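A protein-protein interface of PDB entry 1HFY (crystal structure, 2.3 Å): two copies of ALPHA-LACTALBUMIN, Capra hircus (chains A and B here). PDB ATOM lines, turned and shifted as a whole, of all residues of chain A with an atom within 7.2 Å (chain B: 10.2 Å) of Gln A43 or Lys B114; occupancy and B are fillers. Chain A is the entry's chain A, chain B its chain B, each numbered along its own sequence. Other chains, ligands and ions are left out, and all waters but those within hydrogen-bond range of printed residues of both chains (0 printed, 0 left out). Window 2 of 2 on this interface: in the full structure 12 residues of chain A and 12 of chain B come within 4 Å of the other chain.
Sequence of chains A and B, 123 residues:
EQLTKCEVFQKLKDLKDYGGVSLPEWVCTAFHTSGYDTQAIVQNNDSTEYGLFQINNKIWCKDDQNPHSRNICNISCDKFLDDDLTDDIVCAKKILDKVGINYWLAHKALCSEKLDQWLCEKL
Among the printed residues, pairs that only touch across the chains: Asn A44 with Glu B113 (3.2 Å), Gln A43 with Lys B114 (3.5 Å), Val A42 with Gln B117 (3.7 Å), Val A42 with Phe B31 (3.8 Å) and Asn A44 with Lys B114 (3.996 Å).
Gln A43 touches just these residues of chain B: Lys B114 and Gln B117.
Printed residues of chain A within 4 Å of Lys B114: Gln A43 and Asn A44.
Of the printed residues of chain A, Glu B113 touches Asn A44 and Asn A45.
Of the printed residues of chain A, Phe B31 touches Val A42.
Of the printed residues of chain B, Asn A44 touches Glu B113 (3.2 Å) and Lys B114 (3.996 Å).
Ile A41 touches none of the printed residues of chain B.
Glu A49 touches none of the printed residues of chain B.
The nearest residue of chain B that does not touch Gln A43 is Glu B113 (4.2 Å).
The nearest printed residue of chain A that does not touch Lys B114 is Asn A45 (4.7 Å).
The nearest printed residue of chain A that does not touch Glu B113 is Gln A43 (4.2 Å).
Of the 11 printed residues of chain A, 4 touch a printed residue of chain B.
Hydrophobic or aromatic side chains of chain A within 4 Å of the printed part of chain B: Val A42.
Of the 21 printed residues of chain B, 4 touch a printed residue of chain A.
Printed residues of chain B that touch a printed residue of chain A: Phe B31, Glu B113, Lys B114 and Gln B117.
O of Lys B114 lies close to NE2 of Gln B117 (3.1 Å).
The backbone carbonyl oxygen (O) of Gln B117 lies within hydrogen-bond range of the side-chain amino group (NZ) of Lys B5 (3.2 Å).
The side-chain sulfur (SG) of Cys B111 is disulfide-bonded to the side-chain sulfur (SG) of Cys B28, 2.0 Å away.
The backbone carbonyl oxygen of Glu B113 sits at hydrogen-bond distance from the side-chain amide nitrogen of Gln B117 (3.1 Å).
The side-chain carboxylate of Asp A46 sits close to the side-chain amide oxygen of Asn A45 (2.8 Å).
ND2 of Asn A44 is in hydrogen-bond range of OE1 of Glu A49.
No position is printed for both chains.
Of the 7 pairs that touch across the chains among the printed residues, none has its exchanged pair printed and touching as well.
The side-chain carboxylate (OE2) of Glu B113 sits close to the side-chain amide oxygen (OD1) of Asn A45, at 2.9 Å.
N of Gln A43 is in hydrogen-bond range of OE1 of Gln B117 (3.0 Å).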
ATOM      1  N   ILE A  41      29.314  14.486  23.851  1.00  0.00           N
ATOM      2  CA  ILE A  41      30.114  15.083  22.772  1.00  0.00           C
ATOM      3  C   ILE A  41      29.675  14.452  21.443  1.00  0.00           C
ATOM      4  O   ILE A  41      29.675  13.231  21.301  1.00  0.00           O
ATOM      5  CB  ILE A  41      31.654  14.877  22.995  1.00  0.00           C
ATOM      6  CG1 ILE A  41      32.132  15.680  24.194  1.00  0.00           C
ATOM      7  CG2 ILE A  41      32.463  15.377  21.799  1.00  0.00           C
ATOM      8  CD1 ILE A  41      33.561  15.401  24.519  1.00  0.00           C
ATOM      9  N   VAL A  42      29.275  15.271  20.481  1.00  0.00           N
ATOM     10  CA  VAL A  42      28.848  14.748  19.204  1.00  0.00           C
ATOM     11  C   VAL A  42      29.621  15.445  18.087  1.00  0.00           C
ATOM     12  O   VAL A  42      29.701  16.665  18.047  1.00  0.00           O
ATOM     13  CB  VAL A  42      27.321  14.911  19.052  1.00  0.00           C
ATOM     14  CG1 VAL A  42      26.839  14.473  17.670  1.00  0.00           C
ATOM     15  CG2 VAL A  42      26.639  14.107  20.142  1.00  0.00           C
ATOM     16  N   GLN A  43      30.229  14.658  17.217  1.00  0.00           N
ATOM     17  CA  GLN A  43      31.023  15.182  16.121  1.00  0.00           C
ATOM     18  C   GLN A  43      30.359  15.147  14.749  1.00  0.00           C
ATOM     19  O   GLN A  43      29.488  14.326  14.462  1.00  0.00           O
ATOM     20  CB  GLN A  43      32.347  14.431  16.057  1.00  0.00           C
ATOM     21  CG  GLN A  43      33.238  14.660  17.263  1.00  0.00           C
ATOM     22  CD  GLN A  43      33.951  13.397  17.706  1.00  0.00           C
ATOM     23  OE1 GLN A  43      34.679  12.764  16.925  1.00  0.00           O
ATOM     24  NE2 GLN A  43      33.725  12.999  18.960  1.00  0.00           N
ATOM     25  N   ASN A  44      30.782  16.073  13.908  1.00  0.00           N
ATOM     26  CA  ASN A  44      30.289  16.170  12.551  1.00  0.00           C
ATOM     27  C   ASN A  44      31.553  16.279  11.738  1.00  0.00           C
ATOM     28  O   ASN A  44      32.646  16.369  12.293  1.00  0.00           O
ATOM     29  CB  ASN A  44      29.476  17.439  12.367  1.00  0.00           C
ATOM     30  CG  ASN A  44      28.367  17.550  13.361  1.00  0.00           C
ATOM     31  OD1 ASN A  44      27.385  16.815  13.289  1.00  0.00           O
ATOM     32  ND2 ASN A  44      28.531  18.435  14.339  1.00  0.00           N
ATOM     33  N   ASN A  45      31.419  16.261  10.424  1.00  0.00           N
ATOM     34  CA  ASN A  45      32.591  16.400   9.577  1.00  0.00           C
ATOM     35  C   ASN A  45      33.217  17.755   9.933  1.00  0.00           C
ATOM     36  O   ASN A  45      34.390  17.838  10.301  1.00  0.00           O
ATOM     37  CB  ASN A  45      32.172  16.380   8.100  1.00  0.00           C
ATOM     38  CG  ASN A  45      31.114  17.440   7.778  1.00  0.00           C
ATOM     39  OD1 ASN A  45      30.045  17.480   8.407  1.00  0.00           O
ATOM     40  ND2 ASN A  45      31.430  18.338   6.842  1.00  0.00           N
ATOM     41  N   ASP A  46      32.365  18.776   9.960  1.00  0.00           N
ATOM     42  CA  ASP A  46      32.746  20.157  10.230  1.00  0.00           C
ATOM     43  C   ASP A  46      32.990  20.586  11.698  1.00  0.00           C
ATOM     44  O   ASP A  46      34.035  21.162  12.017  1.00  0.00           O
ATOM     45  CB  ASP A  46      31.716  21.097   9.568  1.00  0.00           C
ATOM     46  CG  ASP A  46      30.288  20.880  10.091  1.00  0.00           C
ATOM     47  OD1 ASP A  46      29.802  19.722  10.124  1.00  0.00           O
ATOM     48  OD2 ASP A  46      29.640  21.878  10.476  1.00  0.00           O
ATOM     49  N   SER A  47      32.046  20.301  12.591  1.00  0.00           N
ATOM     50  CA  SER A  47      32.180  20.723  13.983  1.00  0.00           C
ATOM     51  C   SER A  47      31.986  19.653  15.054  1.00  0.00           C
ATOM     52  O   SER A  47      31.854  18.473  14.768  1.00  0.00           O
ATOM     53  CB  SER A  47      31.203  21.869  14.243  1.00  0.00           C
ATOM     54  OG  SER A  47      29.880  21.467  13.927  1.00  0.00           O
ATOM     55  N   THR A  48      31.992  20.102  16.298  1.00  0.00           N
ATOM     56  CA  THR A  48      31.795  19.263  17.465  1.00  0.00           C
ATOM     57  C   THR A  48      30.871  20.079  18.375  1.00  0.00           C
ATOM     58  O   THR A  48      30.918  21.319  18.355  1.00  0.00           O
ATOM     59  CB  THR A  48      33.128  18.962  18.151  1.00  0.00           C
ATOM     60  OG1 THR A  48      33.960  18.263  17.229  1.00  0.00           O
ATOM     61  CG2 THR A  48      32.933  18.094  19.380  1.00  0.00           C
ATOM     62  N   GLU A  49      30.001  19.390  19.111  1.00  0.00           N
ATOM     63  CA  GLU A  49      29.037  20.033  19.991  1.00  0.00           C
ATOM     64  C   GLU A  49      29.209  19.482  21.364  1.00  0.00           C
ATOM     65  O   GLU A  49      29.343  18.268  21.536  1.00  0.00           O
ATOM     66  CB  GLU A  49      27.641  19.792  19.482  1.00  0.00           C
ATOM     67  CG  GLU A  49      27.336  20.608  18.256  1.00  0.00           C
ATOM     68  CD  GLU A  49      26.320  19.939  17.384  1.00  0.00           C
ATOM     69  OE1 GLU A  49      26.736  18.967  16.710  1.00  0.00           O
ATOM     70  OE2 GLU A  49      25.127  20.363  17.381  1.00  0.00           O
ATOM     71  N   GLN A  54      24.617  20.991  23.864  1.00  0.00           N
ATOM     72  CA  GLN A  54      25.277  20.765  22.588  1.00  0.00           C
ATOM     73  C   GLN A  54      25.751  22.055  21.917  1.00  0.00           C
ATOM     74  O   GLN A  54      25.353  22.371  20.796  1.00  0.00           O
ATOM     75  CB  GLN A  54      24.392  19.936  21.671  1.00  0.00           C
ATOM     76  CG  GLN A  54      24.216  18.496  22.156  1.00  0.00           C
ATOM     77  CD  GLN A  54      25.480  17.658  22.060  1.00  0.00           C
ATOM     78  OE1 GLN A  54      25.782  17.086  21.013  1.00  0.00           O
ATOM     79  NE2 GLN A  54      26.198  17.546  23.158  1.00  0.00           N
ATOM     80  N   GLN A  65      40.433  21.878  17.775  1.00  0.00           N
ATOM     81  CA  GLN A  65      40.001  21.440  16.474  1.00  0.00           C
ATOM     82  C   GLN A  65      39.802  22.674  15.631  1.00  0.00           C
ATOM     83  O   GLN A  65      40.084  22.688  14.445  1.00  0.00           O
ATOM     84  CB  GLN A  65      38.673  20.686  16.596  1.00  0.00           C
ATOM     85  CG  GLN A  65      38.068  20.264  15.250  1.00  0.00           C
ATOM     86  CD  GLN A  65      36.577  19.927  15.330  1.00  0.00           C
ATOM     87  OE1 GLN A  65      36.112  19.341  16.308  1.00  0.00           O
ATOM     88  NE2 GLN A  65      35.823  20.329  14.312  1.00  0.00           N
ATOM     89  N   LYS B   5      26.511   4.411  26.649  1.00  0.00           N
ATOM     90  CA  LYS B   5      26.786   4.114  25.250  1.00  0.00           C
ATOM     91  C   LYS B   5      27.171   2.641  25.075  1.00  0.00           C
ATOM     92  O   LYS B   5      26.645   1.939  24.225  1.00  0.00           O
ATOM     93  CB  LYS B   5      27.929   5.007  24.745  1.00  0.00           C
ATOM     94  CG  LYS B   5      28.150   4.930  23.237  1.00  0.00           C
ATOM     95  CD  LYS B   5      29.313   5.784  22.782  1.00  0.00           C
ATOM     96  CE  LYS B   5      30.640   5.228  23.309  1.00  0.00           C
ATOM     97  NZ  LYS B   5      31.837   5.835  22.621  1.00  0.00           N
ATOM     98  N   SER B  22      24.074  -0.417  10.287  1.00  0.00           N
ATOM     99  CA  SER B  22      25.194  -0.850  11.116  1.00  0.00           C
ATOM    100  C   SER B  22      24.902  -0.632  12.583  1.00  0.00           C
ATOM    101  O   SER B  22      24.026   0.127  12.937  1.00  0.00           O
ATOM    102  CB  SER B  22      26.448  -0.069  10.737  1.00  0.00           C
ATOM    103  OG  SER B  22      26.195   1.325  10.686  1.00  0.00           O
ATOM    104  N   PRO B  24      26.830   0.946  14.930  1.00  0.00           N
ATOM    105  CA  PRO B  24      27.019   2.326  15.393  1.00  0.00           C
ATOM    106  C   PRO B  24      25.872   3.251  14.988  1.00  0.00           C
ATOM    107  O   PRO B  24      25.556   4.209  15.698  1.00  0.00           O
ATOM    108  CB  PRO B  24      28.372   2.712  14.779  1.00  0.00           C
ATOM    109  CG  PRO B  24      28.510   1.760  13.617  1.00  0.00           C
ATOM    110  CD  PRO B  24      28.034   0.496  14.214  1.00  0.00           C
ATOM    111  N   GLU B  25      25.199   2.914  13.892  1.00  0.00           N
ATOM    112  CA  GLU B  25      24.062   3.690  13.434  1.00  0.00           C
ATOM    113  C   GLU B  25      22.852   3.518  14.334  1.00  0.00           C
ATOM    114  O   GLU B  25      22.016   4.388  14.376  1.00  0.00           O
ATOM    115  CB  GLU B  25      23.668   3.280  12.038  1.00  0.00           C
ATOM    116  CG  GLU B  25      24.505   3.877  10.947  1.00  0.00           C
ATOM    117  CD  GLU B  25      23.839   3.721   9.581  1.00  0.00           C
ATOM    118  OE1 GLU B  25      22.635   4.085   9.441  1.00  0.00           O
ATOM    119  OE2 GLU B  25      24.527   3.230   8.656  1.00  0.00           O
ATOM    120  N   VAL B  27      23.060   2.848  17.706  1.00  0.00           N
ATOM    121  CA  VAL B  27      23.485   3.522  18.948  1.00  0.00           C
ATOM    122  C   VAL B  27      23.282   5.032  18.790  1.00  0.00           C
ATOM    123  O   VAL B  27      22.868   5.725  19.705  1.00  0.00           O
ATOM    124  CB  VAL B  27      24.985   3.248  19.235  1.00  0.00           C
ATOM    125  CG1 VAL B  27      25.386   3.809  20.577  1.00  0.00           C
ATOM    126  CG2 VAL B  27      25.266   1.762  19.191  1.00  0.00           C
ATOM    127  N   CYS B  28      23.577   5.530  17.604  1.00  0.00           N
ATOM    128  CA  CYS B  28      23.400   6.936  17.276  1.00  0.00           C
ATOM    129  C   CYS B  28      21.924   7.286  17.311  1.00  0.00           C
ATOM    130  O   CYS B  28      21.532   8.318  17.855  1.00  0.00           O
ATOM    131  CB  CYS B  28      23.936   7.173  15.866  1.00  0.00           C
ATOM    132  SG  CYS B  28      23.865   8.895  15.287  1.00  0.00           S
ATOM    133  N   PHE B  31      20.535   7.328  20.885  1.00  0.00           N
ATOM    134  CA  PHE B  31      20.981   8.538  21.572  1.00  0.00           C
ATOM    135  C   PHE B  31      20.023   9.650  21.252  1.00  0.00           C
ATOM    136  O   PHE B  31      19.448  10.269  22.141  1.00  0.00           O
ATOM    137  CB  PHE B  31      22.362   8.973  21.090  1.00  0.00           C
ATOM    138  CG  PHE B  31      22.812  10.304  21.646  1.00  0.00           C
ATOM    139  CD1 PHE B  31      23.056  10.464  23.009  1.00  0.00           C
ATOM    140  CD2 PHE B  31      22.941  11.414  20.808  1.00  0.00           C
ATOM    141  CE1 PHE B  31      23.417  11.719  23.524  1.00  0.00           C
ATOM    142  CE2 PHE B  31      23.301  12.681  21.318  1.00  0.00           C
ATOM    143  CZ  PHE B  31      23.534  12.828  22.665  1.00  0.00           C
ATOM    144  N   HIS B  32      19.822   9.871  19.967  1.00  0.00           N
ATOM    145  CA  HIS B  32      18.949  10.934  19.507  1.00  0.00           C
ATOM    146  C   HIS B  32      17.452  10.771  19.781  1.00  0.00           C
ATOM    147  O   HIS B  32      16.733  11.764  19.796  1.00  0.00           O
ATOM    148  CB  HIS B  32      19.181  11.181  18.017  1.00  0.00           C
ATOM    149  CG  HIS B  32      20.504  11.811  17.716  1.00  0.00           C
ATOM    150  ND1 HIS B  32      20.773  13.135  17.986  1.00  0.00           N
ATOM    151  CD2 HIS B  32      21.639  11.300  17.176  1.00  0.00           C
ATOM    152  CE1 HIS B  32      22.013  13.411  17.625  1.00  0.00           C
ATOM    153  NE2 HIS B  32      22.560  12.317  17.130  1.00  0.00           N
ATOM    154  N   LYS B 108      18.799  11.038   7.502  1.00  0.00           N
ATOM    155  CA  LYS B 108      19.754   9.965   7.784  1.00  0.00           C
ATOM    156  C   LYS B 108      21.178  10.483   8.002  1.00  0.00           C
ATOM    157  O   LYS B 108      21.968   9.860   8.715  1.00  0.00           O
ATOM    158  CB  LYS B 108      19.727   8.908   6.659  1.00  0.00           C
ATOM    159  CG  LYS B 108      20.529   7.622   6.969  1.00  0.00           C
ATOM    160  CD  LYS B 108      20.157   6.445   6.033  1.00  0.00           C
ATOM    161  CE  LYS B 108      20.728   5.095   6.536  1.00  0.00           C
ATOM    162  NZ  LYS B 108      19.881   3.900   6.172  1.00  0.00           N
ATOM    163  N   ALA B 109      21.482  11.636   7.404  1.00  0.00           N
ATOM    164  CA  ALA B 109      22.793  12.275   7.507  1.00  0.00           C
ATOM    165  C   ALA B 109      23.171  12.483   8.975  1.00  0.00           C
ATOM    166  O   ALA B 109      24.339  12.461   9.358  1.00  0.00           O
ATOM    167  CB  ALA B 109      22.742  13.592   6.804  1.00  0.00           C
ATOM    168  N   LEU B 110      22.148  12.667   9.788  1.00  0.00           N
ATOM    169  CA  LEU B 110      22.296  12.866  11.208  1.00  0.00           C
ATOM    170  C   LEU B 110      23.125  11.754  11.807  1.00  0.00           C
ATOM    171  O   LEU B 110      23.934  11.985  12.704  1.00  0.00           O
ATOM    172  CB  LEU B 110      20.901  12.879  11.818  1.00  0.00           C
ATOM    173  CG  LEU B 110      20.630  13.221  13.273  1.00  0.00           C
ATOM    174  CD1 LEU B 110      20.526  11.958  14.087  1.00  0.00           C
ATOM    175  CD2 LEU B 110      21.708  14.169  13.774  1.00  0.00           C
ATOM    176  N   CYS B 111      22.963  10.546  11.285  1.00  0.00           N
ATOM    177  CA  CYS B 111      23.696   9.421  11.825  1.00  0.00           C
ATOM    178  C   CYS B 111      24.608   8.713  10.839  1.00  0.00           C
ATOM    179  O   CYS B 111      24.694   7.486  10.845  1.00  0.00           O
ATOM    180  CB  CYS B 111      22.735   8.436  12.506  1.00  0.00           C
ATOM    181  SG  CYS B 111      22.183   8.979  14.173  1.00  0.00           S
ATOM    182  N   SER B 112      25.306   9.484  10.006  1.00  0.00           N
ATOM    183  CA  SER B 112      26.243   8.914   9.034  1.00  0.00           C
ATOM    184  C   SER B 112      27.652   9.522   9.080  1.00  0.00           C
ATOM    185  O   SER B 112      28.576   9.003   8.456  1.00  0.00           O
ATOM    186  CB  SER B 112      25.656   8.944   7.607  1.00  0.00           C
ATOM    187  OG  SER B 112      24.954  10.151   7.332  1.00  0.00           O
ATOM    188  N   GLU B 113      27.820  10.596   9.853  1.00  0.00           N
ATOM    189  CA  GLU B 113      29.118  11.260  10.012  1.00  0.00           C
ATOM    190  C   GLU B 113      29.856  10.769  11.260  1.00  0.00           C
ATOM    191  O   GLU B 113      29.287  10.687  12.341  1.00  0.00           O
ATOM    192  CB  GLU B 113      28.952  12.783  10.108  1.00  0.00           C
ATOM    193  CG  GLU B 113      28.572  13.478   8.802  1.00  0.00           C
ATOM    194  CD  GLU B 113      28.250  14.966   8.967  1.00  0.00           C
ATOM    195  OE1 GLU B 113      28.340  15.489  10.098  1.00  0.00           O
ATOM    196  OE2 GLU B 113      27.903  15.617   7.956  1.00  0.00           O
ATOM    197  N   LYS B 114      31.134  10.467  11.103  1.00  0.00           N
ATOM    198  CA  LYS B 114      31.949  10.006  12.210  1.00  0.00           C
ATOM    199  C   LYS B 114      31.297   8.855  12.961  1.00  0.00           C
ATOM    200  O   LYS B 114      31.280   8.885  14.181  1.00  0.00           O
ATOM    201  CB  LYS B 114      32.195  11.161  13.199  1.00  0.00           C
ATOM    202  CG  LYS B 114      32.856  12.390  12.597  1.00  0.00           C
ATOM    203  CD  LYS B 114      34.245  12.055  12.125  1.00  0.00           C
ATOM    204  CE  LYS B 114      35.229  11.974  13.279  1.00  0.00           C
ATOM    205  NZ  LYS B 114      35.671  13.358  13.590  1.00  0.00           N
ATOM    206  N   LEU B 115      30.842   7.815  12.263  1.00  0.00           N
ATOM    207  CA  LEU B 115      30.184   6.685  12.926  1.00  0.00           C
ATOM    208  C   LEU B 115      31.021   5.977  13.958  1.00  0.00           C
ATOM    209  O   LEU B 115      30.501   5.282  14.821  1.00  0.00           O
ATOM    210  CB  LEU B 115      29.675   5.663  11.925  1.00  0.00           C
ATOM    211  CG  LEU B 115      28.408   6.034  11.162  1.00  0.00           C
ATOM    212  CD1 LEU B 115      28.086   4.851  10.283  1.00  0.00           C
ATOM    213  CD2 LEU B 115      27.223   6.374  12.093  1.00  0.00           C
ATOM    214  N   ASP B 116      32.326   6.133  13.855  1.00  0.00           N
ATOM    215  CA  ASP B 116      33.260   5.534  14.806  1.00  0.00           C
ATOM    216  C   ASP B 116      33.157   6.111  16.228  1.00  0.00           C
ATOM    217  O   ASP B 116      33.776   5.590  17.160  1.00  0.00           O
ATOM    218  CB  ASP B 116      34.682   5.721  14.291  1.00  0.00           C
ATOM    219  CG  ASP B 116      34.890   7.103  13.668  1.00  0.00           C
ATOM    220  OD1 ASP B 116      34.507   7.298  12.486  1.00  0.00           O
ATOM    221  OD2 ASP B 116      35.402   7.999  14.375  1.00  0.00           O
ATOM    222  N   GLN B 117      32.391   7.193  16.392  1.00  0.00           N
ATOM    223  CA  GLN B 117      32.212   7.842  17.699  1.00  0.00           C
ATOM    224  C   GLN B 117      31.191   7.073  18.528  1.00  0.00           C
ATOM    225  O   GLN B 117      31.185   7.114  19.766  1.00  0.00           O
ATOM    226  CB  GLN B 117      31.756   9.292  17.512  1.00  0.00           C
ATOM    227  CG  GLN B 117      30.427   9.452  16.799  1.00  0.00           C
ATOM    228  CD  GLN B 117      30.048  10.904  16.588  1.00  0.00           C
ATOM    229  OE1 GLN B 117      30.095  11.704  17.516  1.00  0.00           O
ATOM    230  NE2 GLN B 117      29.691  11.258  15.365  1.00  0.00           N
ATOM    231  N   TRP B 118      30.341   6.343  17.813  1.00  0.00           N
ATOM    232  CA  TRP B 118      29.302   5.540  18.419  1.00  0.00           C
ATOM    233  C   TRP B 118      29.776   4.107  18.703  1.00  0.00           C
ATOM    234  O   TRP B 118      29.002   3.258  19.169  1.00  0.00           O
ATOM    235  CB  TRP B 118      28.100   5.540  17.502  1.00  0.00           C
ATOM    236  CG  TRP B 118      27.669   6.897  17.135  1.00  0.00           C
ATOM    237  CD1 TRP B 118      27.832   7.493  15.936  1.00  0.00           C
ATOM    238  CD2 TRP B 118      26.984   7.842  17.972  1.00  0.00           C
ATOM    239  NE1 TRP B 118      27.292   8.754  15.958  1.00  0.00           N
ATOM    240  CE2 TRP B 118      26.768   8.996  17.202  1.00  0.00           C
ATOM    241  CE3 TRP B 118      26.540   7.823  19.301  1.00  0.00           C
ATOM    242  CZ2 TRP B 118      26.129  10.133  17.710  1.00  0.00           C
ATOM    243  CZ3 TRP B 118      25.905   8.964  19.810  1.00  0.00           C
ATOM    244  CH2 TRP B 118      25.710  10.097  19.015  1.00  0.00           C
ATOM    245  N   LEU B 119      31.054   3.851  18.431  1.00  0.00           N
ATOM    246  CA  LEU B 119      31.652   2.547  18.676  1.00  0.00           C
ATOM    247  C   LEU B 119      32.124   2.470  20.107  1.00  0.00           C
ATOM    248  O   LEU B 119      32.502   3.477  20.699  1.00  0.00           O
ATOM    249  CB  LEU B 119      32.838   2.313  17.752  1.00  0.00           C
ATOM    250  CG  LEU B 119      32.403   1.952  16.350  1.00  0.00           C
ATOM    251  CD1 LEU B 119      33.558   2.102  15.386  1.00  0.00           C
ATOM    252  CD2 LEU B 119      31.888   0.547  16.377  1.00  0.00           C
ATOM    253  N   CYS B 120      32.049   1.272  20.669  1.00  0.00           N
ATOM    254  CA  CYS B 120      32.485   1.025  22.032  1.00  0.00           C
ATOM    255  C   CYS B 120      33.679   0.054  21.960  1.00  0.00           C
ATOM    256  O   CYS B 120      33.492  -1.080  21.435  1.00  0.00           O
ATOM    257  CB  CYS B 120      31.339   0.421  22.852  1.00  0.00           C
ATOM    258  SG  CYS B 120      31.859  -0.174  24.494  1.00  0.00           S
